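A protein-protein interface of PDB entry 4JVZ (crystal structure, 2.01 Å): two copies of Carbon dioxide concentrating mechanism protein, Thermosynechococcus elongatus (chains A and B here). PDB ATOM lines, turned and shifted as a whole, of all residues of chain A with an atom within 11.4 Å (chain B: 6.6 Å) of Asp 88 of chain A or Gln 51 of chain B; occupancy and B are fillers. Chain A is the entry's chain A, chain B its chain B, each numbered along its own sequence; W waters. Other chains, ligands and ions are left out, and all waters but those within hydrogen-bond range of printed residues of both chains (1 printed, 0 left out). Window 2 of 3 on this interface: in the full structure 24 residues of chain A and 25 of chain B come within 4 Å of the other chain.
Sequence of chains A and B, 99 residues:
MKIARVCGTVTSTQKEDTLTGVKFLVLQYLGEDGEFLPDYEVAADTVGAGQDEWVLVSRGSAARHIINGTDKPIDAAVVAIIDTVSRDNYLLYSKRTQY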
ATOM      1  N   THR A  84      16.324 -39.923 -16.730  1.00  0.00           N
ATOM      2  CA  THR A  84      15.228 -39.019 -17.058  1.00  0.00           C
ATOM      3  C   THR A  84      15.630 -37.946 -18.060  1.00  0.00           C
ATOM      4  O   THR A  84      16.798 -37.564 -18.161  1.00  0.00           O
ATOM      5  CB  THR A  84      14.684 -38.287 -15.814  1.00  0.00           C
ATOM      6  OG1 THR A  84      15.632 -37.302 -15.384  1.00  0.00           O
ATOM      7  CG2 THR A  84      14.401 -39.259 -14.689  1.00  0.00           C
ATOM      8  N   VAL A  85      14.635 -37.457 -18.791  1.00  0.00           N
ATOM      9  CA  VAL A  85      14.785 -36.259 -19.601  1.00  0.00           C
ATOM     10  C   VAL A  85      13.522 -35.430 -19.470  1.00  0.00           C
ATOM     11  O   VAL A  85      12.455 -35.830 -19.933  1.00  0.00           O
ATOM     12  CB  VAL A  85      15.023 -36.571 -21.087  1.00  0.00           C
ATOM     13  CG1 VAL A  85      15.195 -35.267 -21.868  1.00  0.00           C
ATOM     14  CG2 VAL A  85      16.235 -37.472 -21.245  1.00  0.00           C
ATOM     15  N   SER A  86      13.649 -34.280 -18.824  1.00  0.00           N
ATOM     16  CA  SER A  86      12.512 -33.414 -18.581  1.00  0.00           C
ATOM     17  C   SER A  86      12.507 -32.261 -19.570  1.00  0.00           C
ATOM     18  O   SER A  86      13.534 -31.628 -19.793  1.00  0.00           O
ATOM     19  CB  SER A  86      12.577 -32.850 -17.164  1.00  0.00           C
ATOM     20  OG  SER A  86      13.700 -31.998 -17.023  1.00  0.00           O
ATOM     21  N   ARG A  87      11.355 -32.001 -20.177  1.00  0.00           N
ATOM     22  CA  ARG A  87      11.153 -30.753 -20.898  1.00  0.00           C
ATOM     23  C   ARG A  87      10.115 -29.915 -20.156  1.00  0.00           C
ATOM     24  O   ARG A  87       9.077 -30.427 -19.738  1.00  0.00           O
ATOM     25  CB  ARG A  87      10.716 -31.001 -22.335  1.00  0.00           C
ATOM     26  CG  ARG A  87      10.600 -29.721 -23.122  1.00  0.00           C
ATOM     27  CD  ARG A  87      10.632 -29.984 -24.608  1.00  0.00           C
ATOM     28  NE  ARG A  87      10.565 -28.750 -25.383  1.00  0.00           N
ATOM     29  CZ  ARG A  87      10.882 -28.661 -26.670  1.00  0.00           C
ATOM     30  NH1 ARG A  87      11.298 -29.735 -27.331  1.00  0.00           N
ATOM     31  NH2 ARG A  87      10.792 -27.498 -27.297  1.00  0.00           N
ATOM     32  N   ASP A  88      10.397 -28.623 -20.019  1.00  0.00           N
ATOM     33  CA  ASP A  88       9.682 -27.766 -19.078  1.00  0.00           C
ATOM     34  C   ASP A  88       9.194 -28.562 -17.862  1.00  0.00           C
ATOM     35  O   ASP A  88      10.001 -28.972 -17.026  1.00  0.00           O
ATOM     36  CB  ASP A  88       8.526 -27.031 -19.763  1.00  0.00           C
ATOM     37  CG  ASP A  88       7.916 -25.959 -18.878  1.00  0.00           C
ATOM     38  OD1 ASP A  88       7.672 -26.238 -17.685  1.00  0.00           O
ATOM     39  OD2 ASP A  88       7.691 -24.835 -19.372  1.00  0.00           O
ATOM     40  N   ASN A  89       7.886 -28.793 -17.770  1.00  0.00           N
ATOM     41  CA  ASN A  89       7.291 -29.371 -16.566  1.00  0.00           C
ATOM     42  C   ASN A  89       6.860 -30.826 -16.725  1.00  0.00           C
ATOM     43  O   ASN A  89       6.061 -31.322 -15.932  1.00  0.00           O
ATOM     44  CB  ASN A  89       6.085 -28.535 -16.125  1.00  0.00           C
ATOM     45  CG  ASN A  89       5.001 -28.471 -17.183  1.00  0.00           C
ATOM     46  OD1 ASN A  89       5.290 -28.302 -18.367  1.00  0.00           O
ATOM     47  ND2 ASN A  89       3.746 -28.603 -16.766  1.00  0.00           N
ATOM     48  N   TYR A  90       7.381 -31.510 -17.739  1.00  0.00           N
ATOM     49  CA  TYR A  90       7.056 -32.920 -17.934  1.00  0.00           C
ATOM     50  C   TYR A  90       8.221 -33.744 -18.462  1.00  0.00           C
ATOM     51  O   TYR A  90       9.249 -33.212 -18.878  1.00  0.00           O
ATOM     52  CB  TYR A  90       5.848 -33.082 -18.863  1.00  0.00           C
ATOM     53  CG  TYR A  90       6.066 -32.593 -20.284  1.00  0.00           C
ATOM     54  CD1 TYR A  90       6.064 -31.236 -20.582  1.00  0.00           C
ATOM     55  CD2 TYR A  90       6.254 -33.487 -21.330  1.00  0.00           C
ATOM     56  CE1 TYR A  90       6.254 -30.787 -21.877  1.00  0.00           C
ATOM     57  CE2 TYR A  90       6.446 -33.043 -22.627  1.00  0.00           C
ATOM     58  CZ  TYR A  90       6.444 -31.696 -22.894  1.00  0.00           C
ATOM     59  OH  TYR A  90       6.634 -31.251 -24.184  1.00  0.00           O
ATOM     60  N   LEU A  91       8.029 -35.058 -18.444  1.00  0.00           N
ATOM     61  CA  LEU A  91       9.053 -35.997 -18.856  1.00  0.00           C
ATOM     62  C   LEU A  91       8.737 -36.566 -20.228  1.00  0.00           C
ATOM     63  O   LEU A  91       7.648 -37.093 -20.452  1.00  0.00           O
ATOM     64  CB  LEU A  91       9.123 -37.145 -17.850  1.00  0.00           C
ATOM     65  CG  LEU A  91       9.140 -36.736 -16.378  1.00  0.00           C
ATOM     66  CD1 LEU A  91       8.837 -37.945 -15.500  1.00  0.00           C
ATOM     67  CD2 LEU A  91      10.476 -36.106 -16.010  1.00  0.00           C
ATOM     68  N   LEU A  92       9.686 -36.452 -21.150  1.00  0.00           N
ATOM     69  CA  LEU A  92       9.601 -37.183 -22.405  1.00  0.00           C
ATOM     70  C   LEU A  92      10.034 -38.622 -22.168  1.00  0.00           C
ATOM     71  O   LEU A  92       9.681 -39.520 -22.932  1.00  0.00           O
ATOM     72  CB  LEU A  92      10.492 -36.547 -23.472  1.00  0.00           C
ATOM     73  CG  LEU A  92      10.037 -35.210 -24.053  1.00  0.00           C
ATOM     74  CD1 LEU A  92      11.044 -34.738 -25.089  1.00  0.00           C
ATOM     75  CD2 LEU A  92       8.640 -35.315 -24.660  1.00  0.00           C
ATOM     76  N   TYR A  93      10.797 -38.836 -21.099  1.00  0.00           N
ATOM     77  CA  TYR A  93      11.360 -40.148 -20.823  1.00  0.00           C
ATOM     78  C   TYR A  93      11.847 -40.282 -19.384  1.00  0.00           C
ATOM     79  O   TYR A  93      12.488 -39.379 -18.848  1.00  0.00           O
ATOM     80  CB  TYR A  93      12.530 -40.401 -21.771  1.00  0.00           C
ATOM     81  CG  TYR A  93      13.246 -41.706 -21.529  1.00  0.00           C
ATOM     82  CD1 TYR A  93      14.199 -41.823 -20.530  1.00  0.00           C
ATOM     83  CD2 TYR A  93      12.972 -42.819 -22.300  1.00  0.00           C
ATOM     84  CE1 TYR A  93      14.855 -43.015 -20.308  1.00  0.00           C
ATOM     85  CE2 TYR A  93      13.621 -44.012 -22.087  1.00  0.00           C
ATOM     86  CZ  TYR A  93      14.565 -44.107 -21.092  1.00  0.00           C
ATOM     87  OH  TYR A  93      15.213 -45.307 -20.870  1.00  0.00           O
ATOM     88  N   ARG B   5      17.594 -21.557 -26.182  1.00  0.00           N
ATOM     89  CA  ARG B   5      16.812 -21.398 -24.962  1.00  0.00           C
ATOM     90  C   ARG B   5      16.735 -22.694 -24.160  1.00  0.00           C
ATOM     91  O   ARG B   5      16.561 -23.779 -24.714  1.00  0.00           O
ATOM     92  CB  ARG B   5      15.399 -20.882 -25.259  1.00  0.00           C
ATOM     93  CG  ARG B   5      14.631 -21.658 -26.313  1.00  0.00           C
ATOM     94  CD  ARG B   5      13.184 -21.196 -26.356  1.00  0.00           C
ATOM     95  NE  ARG B   5      12.365 -21.918 -25.386  1.00  0.00           N
ATOM     96  CZ  ARG B   5      11.667 -23.019 -25.656  1.00  0.00           C
ATOM     97  NH1 ARG B   5      11.667 -23.534 -26.876  1.00  0.00           N
ATOM     98  NH2 ARG B   5      10.955 -23.611 -24.708  1.00  0.00           N
ATOM     99  N   VAL B   6      16.874 -22.556 -22.848  1.00  0.00           N
ATOM    100  CA  VAL B   6      16.813 -23.674 -21.922  1.00  0.00           C
ATOM    101  C   VAL B   6      15.385 -24.206 -21.823  1.00  0.00           C
ATOM    102  O   VAL B   6      14.478 -23.480 -21.424  1.00  0.00           O
ATOM    103  CB  VAL B   6      17.303 -23.215 -20.538  1.00  0.00           C
ATOM    104  CG1 VAL B   6      17.043 -24.275 -19.472  1.00  0.00           C
ATOM    105  CG2 VAL B   6      18.780 -22.834 -20.613  1.00  0.00           C
ATOM    106  N   CYS B   7      15.188 -25.472 -22.182  1.00  0.00           N
ATOM    107  CA  CYS B   7      13.843 -26.043 -22.239  1.00  0.00           C
ATOM    108  C   CYS B   7      13.661 -27.270 -21.345  1.00  0.00           C
ATOM    109  O   CYS B   7      12.536 -27.729 -21.164  1.00  0.00           O
ATOM    110  CB  CYS B   7      13.472 -26.404 -23.684  1.00  0.00           C
ATOM    111  SG  CYS B   7      14.585 -27.591 -24.472  1.00  0.00           S
ATOM    112  N   GLY B   8      14.742 -27.794 -20.770  1.00  0.00           N
ATOM    113  CA  GLY B   8      14.628 -28.988 -19.948  1.00  0.00           C
ATOM    114  C   GLY B   8      15.905 -29.488 -19.288  1.00  0.00           C
ATOM    115  O   GLY B   8      16.896 -28.764 -19.214  1.00  0.00           O
ATOM    116  N   THR B   9      15.875 -30.728 -18.798  1.00  0.00           N
ATOM    117  CA  THR B   9      17.023 -31.303 -18.104  1.00  0.00           C
ATOM    118  C   THR B   9      17.218 -32.785 -18.403  1.00  0.00           C
ATOM    119  O   THR B   9      16.271 -33.495 -18.739  1.00  0.00           O
ATOM    120  CB  THR B   9      16.876 -31.175 -16.578  1.00  0.00           C
ATOM    121  OG1 THR B   9      15.774 -31.977 -16.136  1.00  0.00           O
ATOM    122  CG2 THR B   9      16.654 -29.732 -16.171  1.00  0.00           C
ATOM    123  N   VAL B  26      18.883 -29.402 -21.382  1.00  0.00           N
ATOM    124  CA  VAL B  26      18.327 -29.595 -22.705  1.00  0.00           C
ATOM    125  C   VAL B  26      18.128 -28.215 -23.312  1.00  0.00           C
ATOM    126  O   VAL B  26      17.437 -27.376 -22.739  1.00  0.00           O
ATOM    127  CB  VAL B  26      16.983 -30.331 -22.633  1.00  0.00           C
ATOM    128  CG1 VAL B  26      16.354 -30.449 -24.022  1.00  0.00           C
ATOM    129  CG2 VAL B  26      17.176 -31.697 -21.980  1.00  0.00           C
ATOM    130  N   ALA B  49      22.196 -21.698 -15.612  1.00  0.00           N
ATOM    131  CA  ALA B  49      21.087 -21.279 -16.466  1.00  0.00           C
ATOM    132  C   ALA B  49      19.806 -22.014 -16.080  1.00  0.00           C
ATOM    133  O   ALA B  49      19.853 -23.148 -15.603  1.00  0.00           O
ATOM    134  CB  ALA B  49      21.421 -21.521 -17.938  1.00  0.00           C
ATOM    135  N   GLY B  50      18.665 -21.366 -16.297  1.00  0.00           N
ATOM    136  CA  GLY B  50      17.382 -21.926 -15.913  1.00  0.00           C
ATOM    137  C   GLY B  50      16.373 -21.921 -17.045  1.00  0.00           C
ATOM    138  O   GLY B  50      16.639 -21.415 -18.135  1.00  0.00           O
ATOM    139  N   GLN B  51      15.204 -22.490 -16.769  1.00  0.00           N
ATOM    140  CA  GLN B  51      14.138 -22.640 -17.754  1.00  0.00           C
ATOM    141  C   GLN B  51      13.790 -21.323 -18.461  1.00  0.00           C
ATOM    142  O   GLN B  51      13.610 -20.295 -17.812  1.00  0.00           O
ATOM    143  CB  GLN B  51      12.890 -23.202 -17.063  1.00  0.00           C
ATOM    144  CG  GLN B  51      11.733 -23.502 -17.998  1.00  0.00           C
ATOM    145  CD  GLN B  51      12.036 -24.634 -18.958  1.00  0.00           C
ATOM    146  OE1 GLN B  51      13.008 -25.368 -18.780  1.00  0.00           O
ATOM    147  NE2 GLN B  51      11.208 -24.781 -19.985  1.00  0.00           N
ATOM    148  N   ASP B  52      13.702 -21.373 -19.791  1.00  0.00           N
ATOM    149  CA  ASP B  52      13.255 -20.243 -20.614  1.00  0.00           C
ATOM    150  C   ASP B  52      14.313 -19.166 -20.844  1.00  0.00           C
ATOM    151  O   ASP B  52      14.152 -18.322 -21.722  1.00  0.00           O
ATOM    152  CB  ASP B  52      11.980 -19.621 -20.035  1.00  0.00           C
ATOM    153  CG  ASP B  52      10.787 -20.553 -20.127  1.00  0.00           C
ATOM    154  OD1 ASP B  52      10.666 -21.266 -21.147  1.00  0.00           O
ATOM    155  OD2 ASP B  52       9.970 -20.574 -19.182  1.00  0.00           O
ATOM    156  N   GLU B  53      15.394 -19.197 -20.073  1.00  0.00           N
ATOM    157  CA  GLU B  53      16.473 -18.238 -20.261  1.00  0.00           C
ATOM    158  C   GLU B  53      17.174 -18.481 -21.595  1.00  0.00           C
ATOM    159  O   GLU B  53      17.214 -19.608 -22.089  1.00  0.00           O
ATOM    160  CB  GLU B  53      17.493 -18.339 -19.128  1.00  0.00           C
ATOM    161  CG  GLU B  53      16.961 -17.971 -17.766  1.00  0.00           C
ATOM    162  CD  GLU B  53      18.066 -17.566 -16.815  1.00  0.00           C
ATOM    163  OE1 GLU B  53      18.903 -18.425 -16.471  1.00  0.00           O
ATOM    164  OE2 GLU B  53      18.103 -16.380 -16.424  1.00  0.00           O
HETATM  165  O   HOH W   1      15.239 -34.763 -16.181  1.00  0.00           O
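CA of Val 85 of chain A touches O of Thr 9 of chain B, at 3.3 Å. CA of Gly 8 of chain B touches O of Ser 86 of chain A (2.9 Å). O of Cys 7 of chain B touches CA of Arg 87 of chain A, 3.3 Å away. NE2 of Gln 51 of chain B touches CA of Asp 88 of chain A (3.5 Å).
No position is printed for both chains.
Water W1 lies within hydrogen-bond range of the side-chain hydroxyl of Thr 84 of chain A, the side-chain hydroxyl of Thr 9 of chain B and the backbone NH of Ser 86 of chain A.
Printed residues of chain B that touch a printed residue of chain A: Cys 7, Gly 8, Thr 9 and Gln 51. Along chain B the printed residues that touch a printed residue of chain A span positions 7 to 51. Of the 10 printed residues of chain A, 4 touch a printed residue of chain B. Along chain A the printed residues that touch a printed residue of chain B span positions 85 to 88. Among the printed residues, no Asp or Glu carboxylate lies within 4 Å of a Lys or Arg side-chain nitrogen of the other chain.
The backbone carbonyl oxygen (O) of Val 85 of chain A sits at hydrogen-bond distance from the backbone NH (N) of Leu 92 of chain A (3.1 Å). The backbone carbonyl oxygen of Tyr 93 of chain A sits at hydrogen-bond distance from the backbone NH of Val 85 of chain A, at 2.9 Å. The side-chain carboxylate (OD1) of Asp 88 of chain A lies close to the side-chain amide oxygen (OD1) of Asn 89 of chain A (3.2 Å). The backbone carbonyl oxygen (O) of Val 26 of chain B sits at hydrogen-bond distance from the backbone NH (N) of Cys 7 of chain B, at 3.0 Å. O of Cys 7 of chain B sits close to OE1 of Gln 51 of chain B, at 3.4 Å. N of Val 26 of chain B is in hydrogen-bond range of O of Gly 8 of chain B, at 3.0 Å.
The backbone NH (N) of Thr 9 of chain B is in hydrogen-bond range of the backbone carbonyl oxygen (O) of Ser 86 of chain A (2.7 Å). O of Cys 7 of chain B is in hydrogen-bond range of N of Asp 88 of chain A (2.6 Å).
Asp 88 of chain A touches just these residues of chain B: Cys 7 (2.6 Å) and Gln 51 (3.5 Å). Cys 7 of chain B touches two residues of chain A. No residue of chain A comes within 4 Å of Asp 52 of chain B. No residue of chain A comes within 4 Å of Glu 53 of chain B. Of the printed residues of chain B, Ser 86 of chain A touches Gly 8 (2.9 Å) and Thr 9 (2.3 Å). Printed residues of chain B within 4 Å of Val 85 of chain A: Thr 9. Of the printed residues of chain A, Gly 8 of chain B touches Ser 86 (2.9 Å). The nearest residue of chain B that does not touch Asp 88 of chain A is Gly 8 of chain B (4.2 Å).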
